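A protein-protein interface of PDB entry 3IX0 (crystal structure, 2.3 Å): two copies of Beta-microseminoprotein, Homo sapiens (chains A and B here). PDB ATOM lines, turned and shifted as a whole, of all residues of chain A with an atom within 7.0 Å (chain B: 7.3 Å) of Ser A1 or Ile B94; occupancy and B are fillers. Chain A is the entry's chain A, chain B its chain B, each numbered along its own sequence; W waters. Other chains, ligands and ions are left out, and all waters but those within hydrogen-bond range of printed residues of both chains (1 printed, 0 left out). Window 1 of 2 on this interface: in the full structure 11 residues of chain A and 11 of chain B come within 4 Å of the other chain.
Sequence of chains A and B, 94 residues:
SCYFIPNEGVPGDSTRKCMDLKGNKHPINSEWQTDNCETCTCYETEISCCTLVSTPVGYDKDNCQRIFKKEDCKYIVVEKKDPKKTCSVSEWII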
ATOM      1  N   SER A   1     -12.503  15.171 -26.572  1.00  0.00           N
ATOM      2  CA  SER A   1     -13.369  14.786 -27.657  1.00  0.00           C
ATOM      3  C   SER A   1     -12.831  13.575 -28.431  1.00  0.00           C
ATOM      4  O   SER A   1     -11.653  13.230 -28.351  1.00  0.00           O
ATOM      5  CB  SER A   1     -13.597  15.972 -28.590  1.00  0.00           C
ATOM      6  OG  SER A   1     -14.792  15.797 -29.338  1.00  0.00           O
ATOM      7  N   CYS A   2     -13.719  12.952 -29.195  1.00  0.00           N
ATOM      8  CA  CYS A   2     -13.452  11.669 -29.819  1.00  0.00           C
ATOM      9  C   CYS A   2     -13.901  11.645 -31.278  1.00  0.00           C
ATOM     10  O   CYS A   2     -14.833  12.353 -31.650  1.00  0.00           O
ATOM     11  CB  CYS A   2     -14.225  10.590 -29.073  1.00  0.00           C
ATOM     12  SG  CYS A   2     -14.062  10.571 -27.269  1.00  0.00           S
ATOM     13  N   TYR A   3     -13.235  10.834 -32.100  1.00  0.00           N
ATOM     14  CA  TYR A   3     -13.807  10.439 -33.383  1.00  0.00           C
ATOM     15  C   TYR A   3     -14.160   8.952 -33.365  1.00  0.00           C
ATOM     16  O   TYR A   3     -13.576   8.179 -32.606  1.00  0.00           O
ATOM     17  CB  TYR A   3     -12.893  10.805 -34.565  1.00  0.00           C
ATOM     18  CG  TYR A   3     -11.565  10.070 -34.638  1.00  0.00           C
ATOM     19  CD1 TYR A   3     -11.494   8.787 -35.148  1.00  0.00           C
ATOM     20  CD2 TYR A   3     -10.384  10.679 -34.234  1.00  0.00           C
ATOM     21  CE1 TYR A   3     -10.303   8.106 -35.238  1.00  0.00           C
ATOM     22  CE2 TYR A   3      -9.166  10.001 -34.315  1.00  0.00           C
ATOM     23  CZ  TYR A   3      -9.141   8.707 -34.827  1.00  0.00           C
ATOM     24  OH  TYR A   3      -7.968   7.990 -34.941  1.00  0.00           O
ATOM     25  N   PHE A   4     -15.149   8.582 -34.174  1.00  0.00           N
ATOM     26  CA  PHE A   4     -15.643   7.217 -34.316  1.00  0.00           C
ATOM     27  C   PHE A   4     -15.708   6.896 -35.802  1.00  0.00           C
ATOM     28  O   PHE A   4     -16.384   7.607 -36.561  1.00  0.00           O
ATOM     29  CB  PHE A   4     -17.070   7.100 -33.786  1.00  0.00           C
ATOM     30  CG  PHE A   4     -17.163   7.060 -32.305  1.00  0.00           C
ATOM     31  CD1 PHE A   4     -17.068   8.226 -31.564  1.00  0.00           C
ATOM     32  CD2 PHE A   4     -17.363   5.856 -31.644  1.00  0.00           C
ATOM     33  CE1 PHE A   4     -17.150   8.193 -30.182  1.00  0.00           C
ATOM     34  CE2 PHE A   4     -17.452   5.815 -30.255  1.00  0.00           C
ATOM     35  CZ  PHE A   4     -17.345   6.985 -29.526  1.00  0.00           C
ATOM     36  N   SER A  48     -12.617   3.988 -32.257  1.00  0.00           N
ATOM     37  CA  SER A  48     -12.836   5.231 -31.539  1.00  0.00           C
ATOM     38  C   SER A  48     -11.544   5.776 -30.926  1.00  0.00           C
ATOM     39  O   SER A  48     -10.780   5.037 -30.321  1.00  0.00           O
ATOM     40  CB  SER A  48     -13.853   4.987 -30.435  1.00  0.00           C
ATOM     41  OG  SER A  48     -14.179   6.208 -29.816  1.00  0.00           O
ATOM     42  N   CYS A  49     -11.294   7.070 -31.079  1.00  0.00           N
ATOM     43  CA  CYS A  49     -10.128   7.693 -30.453  1.00  0.00           C
ATOM     44  C   CYS A  49     -10.530   8.996 -29.772  1.00  0.00           C
ATOM     45  O   CYS A  49     -11.260   9.808 -30.351  1.00  0.00           O
ATOM     46  CB  CYS A  49      -9.026   7.964 -31.492  1.00  0.00           C
ATOM     47  SG  CYS A  49      -8.051   6.523 -32.056  1.00  0.00           S
ATOM     48  N   CYS A  50     -10.038   9.206 -28.553  1.00  0.00           N
ATOM     49  CA  CYS A  50     -10.330  10.420 -27.803  1.00  0.00           C
ATOM     50  C   CYS A  50      -9.045  11.001 -27.263  1.00  0.00           C
ATOM     51  O   CYS A  50      -8.120  10.266 -26.910  1.00  0.00           O
ATOM     52  CB  CYS A  50     -11.227  10.124 -26.585  1.00  0.00           C
ATOM     53  SG  CYS A  50     -12.686   9.106 -26.876  1.00  0.00           S
ATOM     54  N   THR A  51      -8.999  12.318 -27.150  1.00  0.00           N
ATOM     55  CA  THR A  51      -7.843  12.960 -26.565  1.00  0.00           C
ATOM     56  C   THR A  51      -7.859  12.797 -25.048  1.00  0.00           C
ATOM     57  O   THR A  51      -8.914  12.825 -24.425  1.00  0.00           O
ATOM     58  CB  THR A  51      -7.784  14.455 -26.946  1.00  0.00           C
ATOM     59  OG1 THR A  51      -6.560  15.018 -26.462  1.00  0.00           O
ATOM     60  CG2 THR A  51      -8.982  15.227 -26.365  1.00  0.00           C
ATOM     61  N   LEU A  52      -6.677  12.627 -24.468  1.00  0.00           N
ATOM     62  CA  LEU A  52      -6.500  12.617 -23.025  1.00  0.00           C
ATOM     63  C   LEU A  52      -6.230  14.007 -22.471  1.00  0.00           C
ATOM     64  O   LEU A  52      -6.130  14.186 -21.248  1.00  0.00           O
ATOM     65  CB  LEU A  52      -5.319  11.713 -22.667  1.00  0.00           C
ATOM     66  CG  LEU A  52      -5.578  10.237 -22.959  1.00  0.00           C
ATOM     67  CD1 LEU A  52      -4.280   9.456 -23.147  1.00  0.00           C
ATOM     68  CD2 LEU A  52      -6.434   9.637 -21.839  1.00  0.00           C
ATOM     69  N   VAL A  53      -6.098  14.994 -23.356  1.00  0.00           N
ATOM     70  CA  VAL A  53      -5.653  16.326 -22.919  1.00  0.00           C
ATOM     71  C   VAL A  53      -6.785  17.313 -22.576  1.00  0.00           C
ATOM     72  O   VAL A  53      -7.604  17.660 -23.433  1.00  0.00           O
ATOM     73  CB  VAL A  53      -4.709  16.979 -23.967  1.00  0.00           C
ATOM     74  CG1 VAL A  53      -4.066  18.208 -23.387  1.00  0.00           C
ATOM     75  CG2 VAL A  53      -3.651  15.996 -24.430  1.00  0.00           C
ATOM     76  N   ILE A  93     -11.242  22.648 -21.094  1.00  0.00           N
ATOM     77  CA  ILE A  93     -12.043  22.002 -22.106  1.00  0.00           C
ATOM     78  C   ILE A  93     -11.347  20.733 -22.544  1.00  0.00           C
ATOM     79  O   ILE A  93     -10.111  20.710 -22.694  1.00  0.00           O
ATOM     80  CB  ILE A  93     -12.225  22.897 -23.321  1.00  0.00           C
ATOM     81  CG1 ILE A  93     -13.242  23.987 -23.013  1.00  0.00           C
ATOM     82  CG2 ILE A  93     -12.740  22.090 -24.491  1.00  0.00           C
ATOM     83  CD1 ILE A  93     -13.741  24.694 -24.248  1.00  0.00           C
ATOM     84  N   ILE A  94     -12.131  19.675 -22.725  1.00  0.00           N
ATOM     85  CA  ILE A  94     -11.602  18.446 -23.307  1.00  0.00           C
ATOM     86  C   ILE A  94     -12.572  17.833 -24.299  1.00  0.00           C
ATOM     87  O   ILE A  94     -13.731  17.551 -23.962  1.00  0.00           O
ATOM     88  CB  ILE A  94     -11.287  17.394 -22.252  1.00  0.00           C
ATOM     89  CG1 ILE A  94     -10.656  16.184 -22.930  1.00  0.00           C
ATOM     90  CG2 ILE A  94     -12.567  16.992 -21.503  1.00  0.00           C
ATOM     91  CD1 ILE A  94     -10.028  15.202 -21.964  1.00  0.00           C
ATOM     92  OXT ILE A  94     -12.187  17.598 -25.442  1.00  0.00           O
ATOM     93  N   SER B   1     -17.248  16.422 -26.195  1.00  0.00           N
ATOM     94  CA  SER B   1     -16.495  17.559 -25.704  1.00  0.00           C
ATOM     95  C   SER B   1     -17.099  18.005 -24.381  1.00  0.00           C
ATOM     96  O   SER B   1     -18.319  18.024 -24.222  1.00  0.00           O
ATOM     97  CB  SER B   1     -16.508  18.705 -26.723  1.00  0.00           C
ATOM     98  OG  SER B   1     -17.827  19.025 -27.145  1.00  0.00           O
ATOM     99  N   CYS B   2     -16.238  18.369 -23.436  1.00  0.00           N
ATOM    100  CA  CYS B   2     -16.683  18.747 -22.105  1.00  0.00           C
ATOM    101  C   CYS B   2     -16.038  20.063 -21.710  1.00  0.00           C
ATOM    102  O   CYS B   2     -14.960  20.402 -22.192  1.00  0.00           O
ATOM    103  CB  CYS B   2     -16.297  17.673 -21.077  1.00  0.00           C
ATOM    104  SG  CYS B   2     -16.731  15.924 -21.484  1.00  0.00           S
ATOM    105  N   CYS B  50     -20.832  17.808 -20.518  1.00  0.00           N
ATOM    106  CA  CYS B  50     -20.381  17.187 -21.747  1.00  0.00           C
ATOM    107  C   CYS B  50     -21.573  17.033 -22.682  1.00  0.00           C
ATOM    108  O   CYS B  50     -22.667  16.725 -22.248  1.00  0.00           O
ATOM    109  CB  CYS B  50     -19.787  15.803 -21.464  1.00  0.00           C
ATOM    110  SG  CYS B  50     -18.414  15.781 -20.330  1.00  0.00           S
ATOM    111  N   THR B  51     -21.358  17.222 -23.978  1.00  0.00           N
ATOM    112  CA  THR B  51     -22.451  17.057 -24.909  1.00  0.00           C
ATOM    113  C   THR B  51     -22.814  15.576 -25.056  1.00  0.00           C
ATOM    114  O   THR B  51     -21.951  14.693 -25.039  1.00  0.00           O
ATOM    115  CB  THR B  51     -22.116  17.640 -26.283  1.00  0.00           C
ATOM    116  OG1 THR B  51     -23.273  17.542 -27.116  1.00  0.00           O
ATOM    117  CG2 THR B  51     -20.975  16.866 -26.934  1.00  0.00           C
ATOM    118  N   LEU B  52     -24.094  15.294 -25.217  1.00  0.00           N
ATOM    119  CA  LEU B  52     -24.473  13.936 -25.588  1.00  0.00           C
ATOM    120  C   LEU B  52     -24.537  13.745 -27.103  1.00  0.00           C
ATOM    121  O   LEU B  52     -24.747  12.635 -27.583  1.00  0.00           O
ATOM    122  CB  LEU B  52     -25.790  13.553 -24.926  1.00  0.00           C
ATOM    123  CG  LEU B  52     -25.638  13.497 -23.402  1.00  0.00           C
ATOM    124  CD1 LEU B  52     -26.984  13.683 -22.714  1.00  0.00           C
ATOM    125  CD2 LEU B  52     -24.952  12.197 -22.980  1.00  0.00           C
ATOM    126  N   VAL B  53     -24.348  14.824 -27.861  1.00  0.00           N
ATOM    127  CA  VAL B  53     -24.608  14.749 -29.298  1.00  0.00           C
ATOM    128  C   VAL B  53     -23.384  14.344 -30.107  1.00  0.00           C
ATOM    129  O   VAL B  53     -22.369  15.024 -30.087  1.00  0.00           O
ATOM    130  CB  VAL B  53     -25.148  16.082 -29.874  1.00  0.00           C
ATOM    131  CG1 VAL B  53     -25.458  15.921 -31.371  1.00  0.00           C
ATOM    132  CG2 VAL B  53     -26.384  16.537 -29.102  1.00  0.00           C
ATOM    133  N   SER B  54     -23.502  13.240 -30.837  1.00  0.00           N
ATOM    134  CA  SER B  54     -22.495  12.859 -31.807  1.00  0.00           C
ATOM    135  C   SER B  54     -22.773  13.492 -33.188  1.00  0.00           C
ATOM    136  O   SER B  54     -23.808  13.248 -33.805  1.00  0.00           O
ATOM    137  CB  SER B  54     -22.436  11.337 -31.921  1.00  0.00           C
ATOM    138  OG  SER B  54     -21.175  10.950 -32.405  1.00  0.00           O
ATOM    139  N   THR B  55     -21.837  14.305 -33.658  1.00  0.00           N
ATOM    140  CA  THR B  55     -21.972  15.014 -34.931  1.00  0.00           C
ATOM    141  C   THR B  55     -21.323  14.241 -36.074  1.00  0.00           C
ATOM    142  O   THR B  55     -20.122  14.012 -36.064  1.00  0.00           O
ATOM    143  CB  THR B  55     -21.291  16.403 -34.845  1.00  0.00           C
ATOM    144  OG1 THR B  55     -21.777  17.086 -33.697  1.00  0.00           O
ATOM    145  CG2 THR B  55     -21.567  17.250 -36.091  1.00  0.00           C
ATOM    146  N   PRO B  56     -22.119  13.837 -37.071  1.00  0.00           N
ATOM    147  CA  PRO B  56     -21.543  13.165 -38.240  1.00  0.00           C
ATOM    148  C   PRO B  56     -20.770  14.168 -39.072  1.00  0.00           C
ATOM    149  O   PRO B  56     -21.299  15.226 -39.370  1.00  0.00           O
ATOM    150  CB  PRO B  56     -22.775  12.713 -39.023  1.00  0.00           C
ATOM    151  CG  PRO B  56     -23.849  13.757 -38.598  1.00  0.00           C
ATOM    152  CD  PRO B  56     -23.591  13.922 -37.136  1.00  0.00           C
ATOM    153  N   TRP B  92     -17.952  10.003 -37.240  1.00  0.00           N
ATOM    154  CA  TRP B  92     -18.694  10.798 -36.271  1.00  0.00           C
ATOM    155  C   TRP B  92     -17.724  11.440 -35.292  1.00  0.00           C
ATOM    156  O   TRP B  92     -16.645  10.909 -35.012  1.00  0.00           O
ATOM    157  CB  TRP B  92     -19.660   9.940 -35.461  1.00  0.00           C
ATOM    158  CG  TRP B  92     -20.725   9.258 -36.236  1.00  0.00           C
ATOM    159  CD1 TRP B  92     -20.608   8.096 -36.950  1.00  0.00           C
ATOM    160  CD2 TRP B  92     -22.090   9.667 -36.355  1.00  0.00           C
ATOM    161  NE1 TRP B  92     -21.814   7.767 -37.512  1.00  0.00           N
ATOM    162  CE2 TRP B  92     -22.741   8.715 -37.164  1.00  0.00           C
ATOM    163  CE3 TRP B  92     -22.820  10.753 -35.864  1.00  0.00           C
ATOM    164  CZ2 TRP B  92     -24.088   8.809 -37.483  1.00  0.00           C
ATOM    165  CZ3 TRP B  92     -24.155  10.848 -36.178  1.00  0.00           C
ATOM    166  CH2 TRP B  92     -24.780   9.881 -36.988  1.00  0.00           C
ATOM    167  N   ILE B  93     -18.129  12.567 -34.732  1.00  0.00           N
ATOM    168  CA  ILE B  93     -17.321  13.218 -33.720  1.00  0.00           C
ATOM    169  C   ILE B  93     -18.190  13.622 -32.551  1.00  0.00           C
ATOM    170  O   ILE B  93     -19.336  14.030 -32.745  1.00  0.00           O
ATOM    171  CB  ILE B  93     -16.608  14.432 -34.303  1.00  0.00           C
ATOM    172  CG1 ILE B  93     -15.301  13.972 -34.954  1.00  0.00           C
ATOM    173  CG2 ILE B  93     -16.369  15.474 -33.220  1.00  0.00           C
ATOM    174  CD1 ILE B  93     -14.471  15.068 -35.547  1.00  0.00           C
ATOM    175  N   ILE B  94     -17.660  13.487 -31.338  1.00  0.00           N
ATOM    176  CA  ILE B  94     -18.383  13.902 -30.142  1.00  0.00           C
ATOM    177  C   ILE B  94     -17.469  14.408 -29.045  1.00  0.00           C
ATOM    178  O   ILE B  94     -16.580  13.685 -28.585  1.00  0.00           O
ATOM    179  CB  ILE B  94     -19.225  12.778 -29.545  1.00  0.00           C
ATOM    180  CG1 ILE B  94     -20.126  13.347 -28.451  1.00  0.00           C
ATOM    181  CG2 ILE B  94     -18.337  11.682 -28.957  1.00  0.00           C
ATOM    182  CD1 ILE B  94     -20.993  12.304 -27.799  1.00  0.00           C
ATOM    183  OXT ILE B  94     -17.635  15.543 -28.596  1.00  0.00           O
HETATM  184  O   HOH W   1     -15.275  14.702 -25.370  1.00  0.00           O
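The backbone NH of Phe A4 is in hydrogen-bond range of the backbone carbonyl oxygen of Trp B92, 2.9 Å away. N of Cys A2 sits at hydrogen-bond distance from O of Ile B94. The chain-end carboxylate of Ile A94 is in hydrogen-bond range of the backbone NH of Cys B2, at 2.7 Å. OG of Ser A1 sits at hydrogen-bond distance from O of Ile B94 (2.9 Å).
N of Ser B1 lies within hydrogen-bond range of OXT of Ile B94. O of Ser A1 is in hydrogen-bond range of N of Thr A51, 3.1 Å away. The backbone NH (N) of Ser A1 is in hydrogen-bond range of the chain-end carboxylate (OXT) of Ile A94, 2.7 Å away. The side-chain sulfur (SG) of Cys A2 forms a disulfide with the side-chain sulfur (SG) of Cys A50 (2.0 Å). The side-chain sulfur (SG) of Cys B2 forms a disulfide with the side-chain sulfur (SG) of Cys B50. O of Cys A49 sits at hydrogen-bond distance from N of Tyr A3, 2.8 Å away.
O of Cys A2 touches CA of Ile B93 (3.4 Å). Trp B92 touches Tyr A3. Ile B93 touches Tyr A3. Ile B94 touches Phe A4. Ile A93 touches Cys B2. O of Ile A94 touches CA of Ser B1, 3.3 Å away.
Ser A1 touches one residue of chain B. Printed residues of chain B within 4 Å of Cys A2: Ile B93 (3.4 Å) and Ile B94 (3.0 Å). Printed residues of chain A within 4 Å of Trp B92: Tyr A3 (3.3 Å) and Phe A4 (2.9 Å). Of the printed residues of chain A, Ile B93 touches Cys A2 (3.4 Å) and Tyr A3 (3.997 Å). Ile B94 touches just these residues of chain A: Ser A1, Cys A2 and Phe A4. The nearest residue of chain B that does not touch Ser A1 is Ser B1 (4.04 Å). The nearest printed residue of chain B that does not touch Ile A94 is Cys B50 (6.1 Å).
Hydrophobic or aromatic side chains of chain B that line the printed part of chain A: Ile B93 and Ile B94. Of the 12 printed residues of chain A, 6 touch a printed residue of chain B. Among the printed residues, 10 pairs touch across the chains. Among the printed residues, no Asp or Glu carboxylate lies within 4 Å of a Lys or Arg side-chain nitrogen of the other chain.
Ser A1 touches Ile B94, and with the chains exchanged Ile A94 touches Ser B1. Cys A2 touches Ile B93, and with the chains exchanged Ile A93 touches Cys B2. Cys A2 touches Ile B94, and with the chains exchanged Ile A94 touches Cys B2. Positions printed for both chains: 1, 2, 50, 51, 52, 53, 93 and 94. Of the 10 pairs that touch across the chains among the printed residues, 6 have their exchanged pair printed and touching as well.
Water W1 bridges the backbone NH (N) of Ser B1 (2.7 Å) and the backbone NH (N) of Ser A1 (3.1 Å).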
